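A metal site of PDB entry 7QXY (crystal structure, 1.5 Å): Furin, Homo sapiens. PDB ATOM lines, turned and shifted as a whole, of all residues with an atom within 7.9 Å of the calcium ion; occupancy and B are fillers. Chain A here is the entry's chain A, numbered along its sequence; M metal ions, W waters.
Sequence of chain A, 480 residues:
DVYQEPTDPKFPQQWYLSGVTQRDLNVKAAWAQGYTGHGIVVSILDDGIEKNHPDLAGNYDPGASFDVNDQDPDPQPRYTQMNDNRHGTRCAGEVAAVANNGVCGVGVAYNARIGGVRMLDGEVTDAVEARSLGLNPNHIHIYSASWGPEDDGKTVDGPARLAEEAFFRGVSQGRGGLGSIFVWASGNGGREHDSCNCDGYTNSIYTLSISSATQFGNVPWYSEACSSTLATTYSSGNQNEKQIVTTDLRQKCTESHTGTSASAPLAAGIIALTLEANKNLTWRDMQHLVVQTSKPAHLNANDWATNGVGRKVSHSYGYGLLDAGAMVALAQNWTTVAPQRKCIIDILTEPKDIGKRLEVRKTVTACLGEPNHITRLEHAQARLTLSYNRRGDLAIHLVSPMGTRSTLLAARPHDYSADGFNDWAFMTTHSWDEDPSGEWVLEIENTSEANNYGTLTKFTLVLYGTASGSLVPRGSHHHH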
ATOM      1  N   GLY A 148      -7.145  30.533  -2.285  1.00  0.00           N
ATOM      2  CA  GLY A 148      -6.451  29.994  -1.126  1.00  0.00           C
ATOM      3  C   GLY A 148      -4.978  29.883  -1.433  1.00  0.00           C
ATOM      4  O   GLY A 148      -4.433  30.638  -2.244  1.00  0.00           O
ATOM      5  N   PRO A 149      -4.308  28.893  -0.831  1.00  0.00           N
ATOM      6  CA  PRO A 149      -2.881  28.699  -1.099  1.00  0.00           C
ATOM      7  C   PRO A 149      -2.606  28.460  -2.580  1.00  0.00           C
ATOM      8  O   PRO A 149      -3.479  28.008  -3.316  1.00  0.00           O
ATOM      9  CB  PRO A 149      -2.519  27.448  -0.289  1.00  0.00           C
ATOM     10  CG  PRO A 149      -3.590  27.301   0.705  1.00  0.00           C
ATOM     11  CD  PRO A 149      -4.827  27.922   0.145  1.00  0.00           C
ATOM     12  N   GLU A 150      -1.372  28.719  -3.014  1.00  0.00           N
ATOM     13  CA  GLU A 150      -1.017  28.601  -4.431  1.00  0.00           C
ATOM     14  C   GLU A 150      -1.426  27.256  -5.057  1.00  0.00           C
ATOM     15  O   GLU A 150      -1.195  26.209  -4.464  1.00  0.00           O
ATOM     16  CB  GLU A 150       0.483  28.824  -4.629  1.00  0.00           C
ATOM     17  CG  GLU A 150       0.853  29.100  -6.073  1.00  0.00           C
ATOM     18  CD  GLU A 150       2.303  29.500  -6.289  1.00  0.00           C
ATOM     19  OE1 GLU A 150       3.030  29.684  -5.289  1.00  0.00           O
ATOM     20  OE2 GLU A 150       2.718  29.617  -7.474  1.00  0.00           O
ATOM     21  N   ASP A 151      -2.061  27.322  -6.233  1.00  0.00           N
ATOM     22  CA  ASP A 151      -2.530  26.142  -6.956  1.00  0.00           C
ATOM     23  C   ASP A 151      -1.445  25.676  -7.914  1.00  0.00           C
ATOM     24  O   ASP A 151      -1.707  25.421  -9.087  1.00  0.00           O
ATOM     25  CB  ASP A 151      -3.831  26.477  -7.699  1.00  0.00           C
ATOM     26  CG  ASP A 151      -5.043  26.572  -6.788  1.00  0.00           C
ATOM     27  OD1 ASP A 151      -5.030  25.934  -5.716  1.00  0.00           O
ATOM     28  OD2 ASP A 151      -6.051  27.212  -7.193  1.00  0.00           O
ATOM     29  N   ASP A 152      -0.209  25.576  -7.411  1.00  0.00           N
ATOM     30  CA  ASP A 152       0.939  25.142  -8.222  1.00  0.00           C
ATOM     31  C   ASP A 152       1.156  23.617  -8.227  1.00  0.00           C
ATOM     32  O   ASP A 152       2.075  23.140  -8.894  1.00  0.00           O
ATOM     33  CB  ASP A 152       2.229  25.858  -7.777  1.00  0.00           C
ATOM     34  CG  ASP A 152       2.610  25.717  -6.318  1.00  0.00           C
ATOM     35  OD1 ASP A 152       1.929  24.958  -5.590  1.00  0.00           O
ATOM     36  OD2 ASP A 152       3.611  26.353  -5.897  1.00  0.00           O
ATOM     37  N   GLY A 153       0.360  22.861  -7.480  1.00  0.00           N
ATOM     38  CA  GLY A 153       0.522  21.412  -7.405  1.00  0.00           C
ATOM     39  C   GLY A 153       1.696  20.963  -6.560  1.00  0.00           C
ATOM     40  O   GLY A 153       2.095  19.791  -6.627  1.00  0.00           O
ATOM     41  N   LYS A 154       2.271  21.878  -5.757  1.00  0.00           N
ATOM     42  CA  LYS A 154       3.357  21.518  -4.855  1.00  0.00           C
ATOM     43  C   LYS A 154       3.229  22.088  -3.453  1.00  0.00           C
ATOM     44  O   LYS A 154       4.023  21.719  -2.605  1.00  0.00           O
ATOM     45  CB  LYS A 154       4.709  21.867  -5.470  1.00  0.00           C
ATOM     46  CG  LYS A 154       4.953  23.334  -5.638  1.00  0.00           C
ATOM     47  CD  LYS A 154       6.325  23.637  -6.244  1.00  0.00           C
ATOM     48  CE  LYS A 154       6.332  23.495  -7.734  1.00  0.00           C
ATOM     49  N   THR A 155       2.200  22.873  -3.171  1.00  0.00           N
ATOM     50  CA  THR A 155       2.027  23.496  -1.865  1.00  0.00           C
ATOM     51  C   THR A 155       1.131  22.669  -0.963  1.00  0.00           C
ATOM     52  O   THR A 155       0.111  22.123  -1.421  1.00  0.00           O
ATOM     53  CB  THR A 155       1.406  24.895  -2.093  1.00  0.00           C
ATOM     54  OG1 THR A 155       2.322  25.648  -2.915  1.00  0.00           O
ATOM     55  CG2 THR A 155       1.141  25.648  -0.788  1.00  0.00           C
ATOM     56  N   ALA A 185     -14.172  27.711  -2.948  1.00  0.00           N
ATOM     57  CA  ALA A 185     -13.895  27.077  -4.224  1.00  0.00           C
ATOM     58  C   ALA A 185     -12.819  26.015  -3.956  1.00  0.00           C
ATOM     59  O   ALA A 185     -11.835  26.310  -3.261  1.00  0.00           O
ATOM     60  CB  ALA A 185     -13.339  28.115  -5.211  1.00  0.00           C
ATOM     61  N   SER A 186     -12.944  24.814  -4.565  1.00  0.00           N
ATOM     62  CA  SER A 186     -11.951  23.762  -4.318  1.00  0.00           C
ATOM     63  C   SER A 186     -10.593  23.980  -5.003  1.00  0.00           C
ATOM     64  O   SER A 186      -9.636  23.276  -4.667  1.00  0.00           O
ATOM     65  CB  SER A 186     -12.523  22.406  -4.696  1.00  0.00           C
ATOM     66  OG  SER A 186     -12.861  22.376  -6.073  1.00  0.00           O
ATOM     67  N   GLY A 187     -10.498  24.942  -5.931  1.00  0.00           N
ATOM     68  CA  GLY A 187      -9.202  25.264  -6.536  1.00  0.00           C
ATOM     69  C   GLY A 187      -9.187  25.276  -8.060  1.00  0.00           C
ATOM     70  O   GLY A 187     -10.095  24.723  -8.707  1.00  0.00           O
ATOM     71  N   ASN A 188      -8.139  25.904  -8.630  1.00  0.00           N
ATOM     72  CA  ASN A 188      -7.947  26.016 -10.082  1.00  0.00           C
ATOM     73  C   ASN A 188      -6.647  25.326 -10.547  1.00  0.00           C
ATOM     74  O   ASN A 188      -6.183  25.607 -11.663  1.00  0.00           O
ATOM     75  CB  ASN A 188      -7.872  27.505 -10.513  1.00  0.00           C
ATOM     76  CG  ASN A 188      -9.166  28.252 -10.275  1.00  0.00           C
ATOM     77  OD1 ASN A 188     -10.239  27.740 -10.553  1.00  0.00           O
ATOM     78  ND2 ASN A 188      -9.092  29.503  -9.806  1.00  0.00           N
ATOM     79  N   GLY A 189      -6.085  24.417  -9.740  1.00  0.00           N
ATOM     80  CA  GLY A 189      -4.794  23.792 -10.028  1.00  0.00           C
ATOM     81  C   GLY A 189      -4.814  22.539 -10.869  1.00  0.00           C
ATOM     82  O   GLY A 189      -3.830  21.806 -10.900  1.00  0.00           O
ATOM     83  N   GLY A 190      -5.893  22.309 -11.601  1.00  0.00           N
ATOM     84  CA  GLY A 190      -6.020  21.111 -12.430  1.00  0.00           C
ATOM     85  C   GLY A 190      -4.871  20.870 -13.403  1.00  0.00           C
ATOM     86  O   GLY A 190      -4.395  19.729 -13.492  1.00  0.00           O
ATOM     87  N   HIS A 193      -1.899  19.291 -11.895  1.00  0.00           N
ATOM     88  CA  HIS A 193      -2.213  18.027 -11.214  1.00  0.00           C
ATOM     89  C   HIS A 193      -2.330  18.245  -9.719  1.00  0.00           C
ATOM     90  O   HIS A 193      -1.965  17.356  -8.951  1.00  0.00           O
ATOM     91  CB  HIS A 193      -1.141  16.989 -11.564  1.00  0.00           C
ATOM     92  CG  HIS A 193      -1.017  16.781 -13.037  1.00  0.00           C
ATOM     93  ND1 HIS A 193       0.099  17.204 -13.742  1.00  0.00           N
ATOM     94  CD2 HIS A 193      -1.926  16.318 -13.917  1.00  0.00           C
ATOM     95  CE1 HIS A 193      -0.155  16.949 -15.014  1.00  0.00           C
ATOM     96  NE2 HIS A 193      -1.358  16.418 -15.167  1.00  0.00           N
ATOM     97  N   ASP A 194      -2.886  19.388  -9.297  1.00  0.00           N
ATOM     98  CA  ASP A 194      -3.048  19.645  -7.869  1.00  0.00           C
ATOM     99  C   ASP A 194      -4.188  18.756  -7.316  1.00  0.00           C
ATOM    100  O   ASP A 194      -5.077  18.330  -8.052  1.00  0.00           O
ATOM    101  CB  ASP A 194      -3.329  21.138  -7.636  1.00  0.00           C
ATOM    102  CG  ASP A 194      -3.011  21.656  -6.245  1.00  0.00           C
ATOM    103  OD1 ASP A 194      -2.528  20.853  -5.410  1.00  0.00           O
ATOM    104  OD2 ASP A 194      -3.289  22.853  -5.976  1.00  0.00           O
ATOM    105  N   SER A 195      -4.133  18.473  -6.005  1.00  0.00           N
ATOM    106  CA  SER A 195      -5.051  17.580  -5.276  1.00  0.00           C
ATOM    107  C   SER A 195      -5.567  18.462  -4.148  1.00  0.00           C
ATOM    108  O   SER A 195      -4.762  18.915  -3.348  1.00  0.00           O
ATOM    109  CB  SER A 195      -4.230  16.377  -4.775  1.00  0.00           C
ATOM    110  OG  SER A 195      -4.978  15.211  -4.458  1.00  0.00           O
ATOM    111  N   CYS A 196      -6.883  18.800  -4.119  1.00  0.00           N
ATOM    112  CA  CYS A 196      -7.367  19.852  -3.222  1.00  0.00           C
ATOM    113  C   CYS A 196      -7.350  19.528  -1.709  1.00  0.00           C
ATOM    114  O   CYS A 196      -7.545  20.484  -0.929  1.00  0.00           O
ATOM    115  CB  CYS A 196      -8.728  20.426  -3.657  1.00  0.00           C
ATOM    116  SG  CYS A 196      -9.897  19.253  -4.405  1.00  0.00           S
ATOM    117  N   ASN A 197      -7.080  18.277  -1.262  1.00  0.00           N
ATOM    118  CA  ASN A 197      -6.971  18.060   0.202  1.00  0.00           C
ATOM    119  C   ASN A 197      -5.672  18.701   0.740  1.00  0.00           C
ATOM    120  O   ASN A 197      -5.543  18.846   1.965  1.00  0.00           O
ATOM    121  CB  ASN A 197      -7.035  16.587   0.577  1.00  0.00           C
ATOM    122  CG  ASN A 197      -8.425  16.013   0.436  1.00  0.00           C
ATOM    123  OD1 ASN A 197      -9.436  16.715   0.258  1.00  0.00           O
ATOM    124  ND2 ASN A 197      -8.514  14.703   0.540  1.00  0.00           N
ATOM    125  N   CYS A 198      -4.721  19.105  -0.143  1.00  0.00           N
ATOM    126  CA  CYS A 198      -3.526  19.843   0.280  1.00  0.00           C
ATOM    127  C   CYS A 198      -3.797  21.323   0.543  1.00  0.00           C
ATOM    128  O   CYS A 198      -2.854  22.044   0.816  1.00  0.00           O
ATOM    129  CB  CYS A 198      -2.420  19.671  -0.747  1.00  0.00           C
ATOM    130  SG  CYS A 198      -1.897  17.959  -0.932  1.00  0.00           S
ATOM    131  N   ASP A 199      -5.047  21.797   0.401  1.00  0.00           N
ATOM    132  CA  ASP A 199      -5.449  23.189   0.638  1.00  0.00           C
ATOM    133  C   ASP A 199      -6.317  23.093   1.877  1.00  0.00           C
ATOM    134  O   ASP A 199      -7.413  22.559   1.803  1.00  0.00           O
ATOM    135  CB  ASP A 199      -6.222  23.701  -0.605  1.00  0.00           C
ATOM    136  CG  ASP A 199      -7.028  24.993  -0.438  1.00  0.00           C
ATOM    137  OD1 ASP A 199      -7.246  25.421   0.715  1.00  0.00           O
ATOM    138  OD2 ASP A 199      -7.479  25.553  -1.484  1.00  0.00           O
ATOM    139  N   THR A 202     -10.244  24.624   1.777  1.00  0.00           N
ATOM    140  CA  THR A 202     -11.310  23.797   1.180  1.00  0.00           C
ATOM    141  C   THR A 202     -11.391  22.442   1.923  1.00  0.00           C
ATOM    142  O   THR A 202     -12.487  21.898   2.106  1.00  0.00           O
ATOM    143  CB  THR A 202     -11.108  23.664  -0.329  1.00  0.00           C
ATOM    144  OG1 THR A 202     -12.285  23.087  -0.906  1.00  0.00           O
ATOM    145  CG2 THR A 202      -9.883  22.806  -0.665  1.00  0.00           C
ATOM    146  N   TYR A 222      -9.157  23.033 -15.329  1.00  0.00           N
ATOM    147  CA  TYR A 222      -8.640  23.631 -14.084  1.00  0.00           C
ATOM    148  C   TYR A 222      -9.113  22.929 -12.813  1.00  0.00           C
ATOM    149  O   TYR A 222      -8.660  23.284 -11.723  1.00  0.00           O
ATOM    150  CB  TYR A 222      -9.042  25.129 -14.010  1.00  0.00           C
ATOM    151  CG  TYR A 222     -10.529  25.352 -14.208  1.00  0.00           C
ATOM    152  CD1 TYR A 222     -11.430  25.128 -13.185  1.00  0.00           C
ATOM    153  CD2 TYR A 222     -11.026  25.819 -15.421  1.00  0.00           C
ATOM    154  CE1 TYR A 222     -12.806  25.231 -13.388  1.00  0.00           C
ATOM    155  CE2 TYR A 222     -12.390  25.967 -15.637  1.00  0.00           C
ATOM    156  CZ  TYR A 222     -13.272  25.697 -14.605  1.00  0.00           C
ATOM    157  OH  TYR A 222     -14.640  25.802 -14.779  1.00  0.00           O
ATOM    158  N   GLU A 224      -9.640  20.524  -9.590  1.00  0.00           N
ATOM    159  CA  GLU A 224      -8.824  19.689  -8.705  1.00  0.00           C
ATOM    160  C   GLU A 224      -9.735  18.642  -8.125  1.00  0.00           C
ATOM    161  O   GLU A 224     -10.821  18.983  -7.664  1.00  0.00           O
ATOM    162  CB  GLU A 224      -8.237  20.504  -7.539  1.00  0.00           C
ATOM    163  CG  GLU A 224      -7.292  21.589  -8.017  1.00  0.00           C
ATOM    164  CD  GLU A 224      -6.617  22.351  -6.887  1.00  0.00           C
ATOM    165  OE1 GLU A 224      -6.354  23.562  -7.082  1.00  0.00           O
ATOM    166  OE2 GLU A 224      -6.324  21.756  -5.826  1.00  0.00           O
ATOM    167  N   ARG A 412       1.128  13.984  -7.038  1.00  0.00           N
ATOM    168  CA  ARG A 412       1.301  15.365  -7.475  1.00  0.00           C
ATOM    169  C   ARG A 412       2.711  15.452  -8.057  1.00  0.00           C
ATOM    170  O   ARG A 412       3.677  15.628  -7.306  1.00  0.00           O
ATOM    171  CB  ARG A 412       1.132  16.327  -6.289  1.00  0.00           C
ATOM    172  CG  ARG A 412      -0.334  16.436  -5.818  1.00  0.00           C
ATOM    173  CD  ARG A 412      -0.623  17.746  -5.117  1.00  0.00           C
ATOM    174  NE  ARG A 412       0.307  17.986  -4.008  1.00  0.00           N
ATOM    175  CZ  ARG A 412       0.438  19.152  -3.377  1.00  0.00           C
ATOM    176  NH1 ARG A 412       1.333  19.280  -2.399  1.00  0.00           N
ATOM    177  NH2 ARG A 412      -0.306  20.187  -3.716  1.00  0.00           N
HETATM  178 CA    CA M   1      -5.179  23.688  -4.916  1.00  0.00          CA
HETATM  179  O   HOH W   1      -7.163  24.053  -3.780  1.00  0.00           O
HETATM  180  O   HOH W   2      -4.363  22.046  -3.302  1.00  0.00           O
HETATM  181  O   HOH W   3      -3.886  24.984  -3.299  1.00  0.00           O
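Within 4 Å of the calcium ion: Asp 151, Asp 194 and Glu 224.
The nearest printed residue that does not touch the calcium ion is Asp 199 (4.4 Å).
The calcium ion is bound by water W1, at 2.3 Å.
The side-chain carboxylate (OD2) of Asp 194 is bound to the calcium ion (2.3 Å).
OD1 of Asp 151 binds the calcium ion.
The side-chain carboxylate (OE2) of Glu 224 is bound to the calcium ion (2.4 Å).
The calcium ion is bound by water W2 (2.4 Å).
Water W3 is bound to the calcium ion, 2.4 Å away.
OE1 of Glu 224 binds the calcium ion (2.5 Å).
The calcium ion has seven donor atoms within binding distance.
O of Gly 189 is in hydrogen-bond range of N of Asp 194, 3.1 Å away.
The side-chain carboxylate (OD2) of Asp 151 is in hydrogen-bond range of the backbone NH (N) of Asn 188, at 2.9 Å.
OD1 of Asp 194 lies within salt-bridge range of NH2 of Arg 412.
The side-chain carboxylate (OE2) of Glu 224 sits close to the backbone NH (N) of Cys 196, 3.5 Å away.
The side-chain carboxylate of Glu 224 lies close to the backbone NH of Asn 188.
The side-chain carboxylate (OE1) of Glu 224 lies close to the backbone NH (N) of Gly 189.
Water W1 lies within hydrogen-bond range of O of Ser 186 and OD2 of Asp 199.
Water W2 lies within hydrogen-bond range of the side-chain carboxylate (OD1) of Asp 194 and the backbone carbonyl oxygen (O) of Ser 195.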
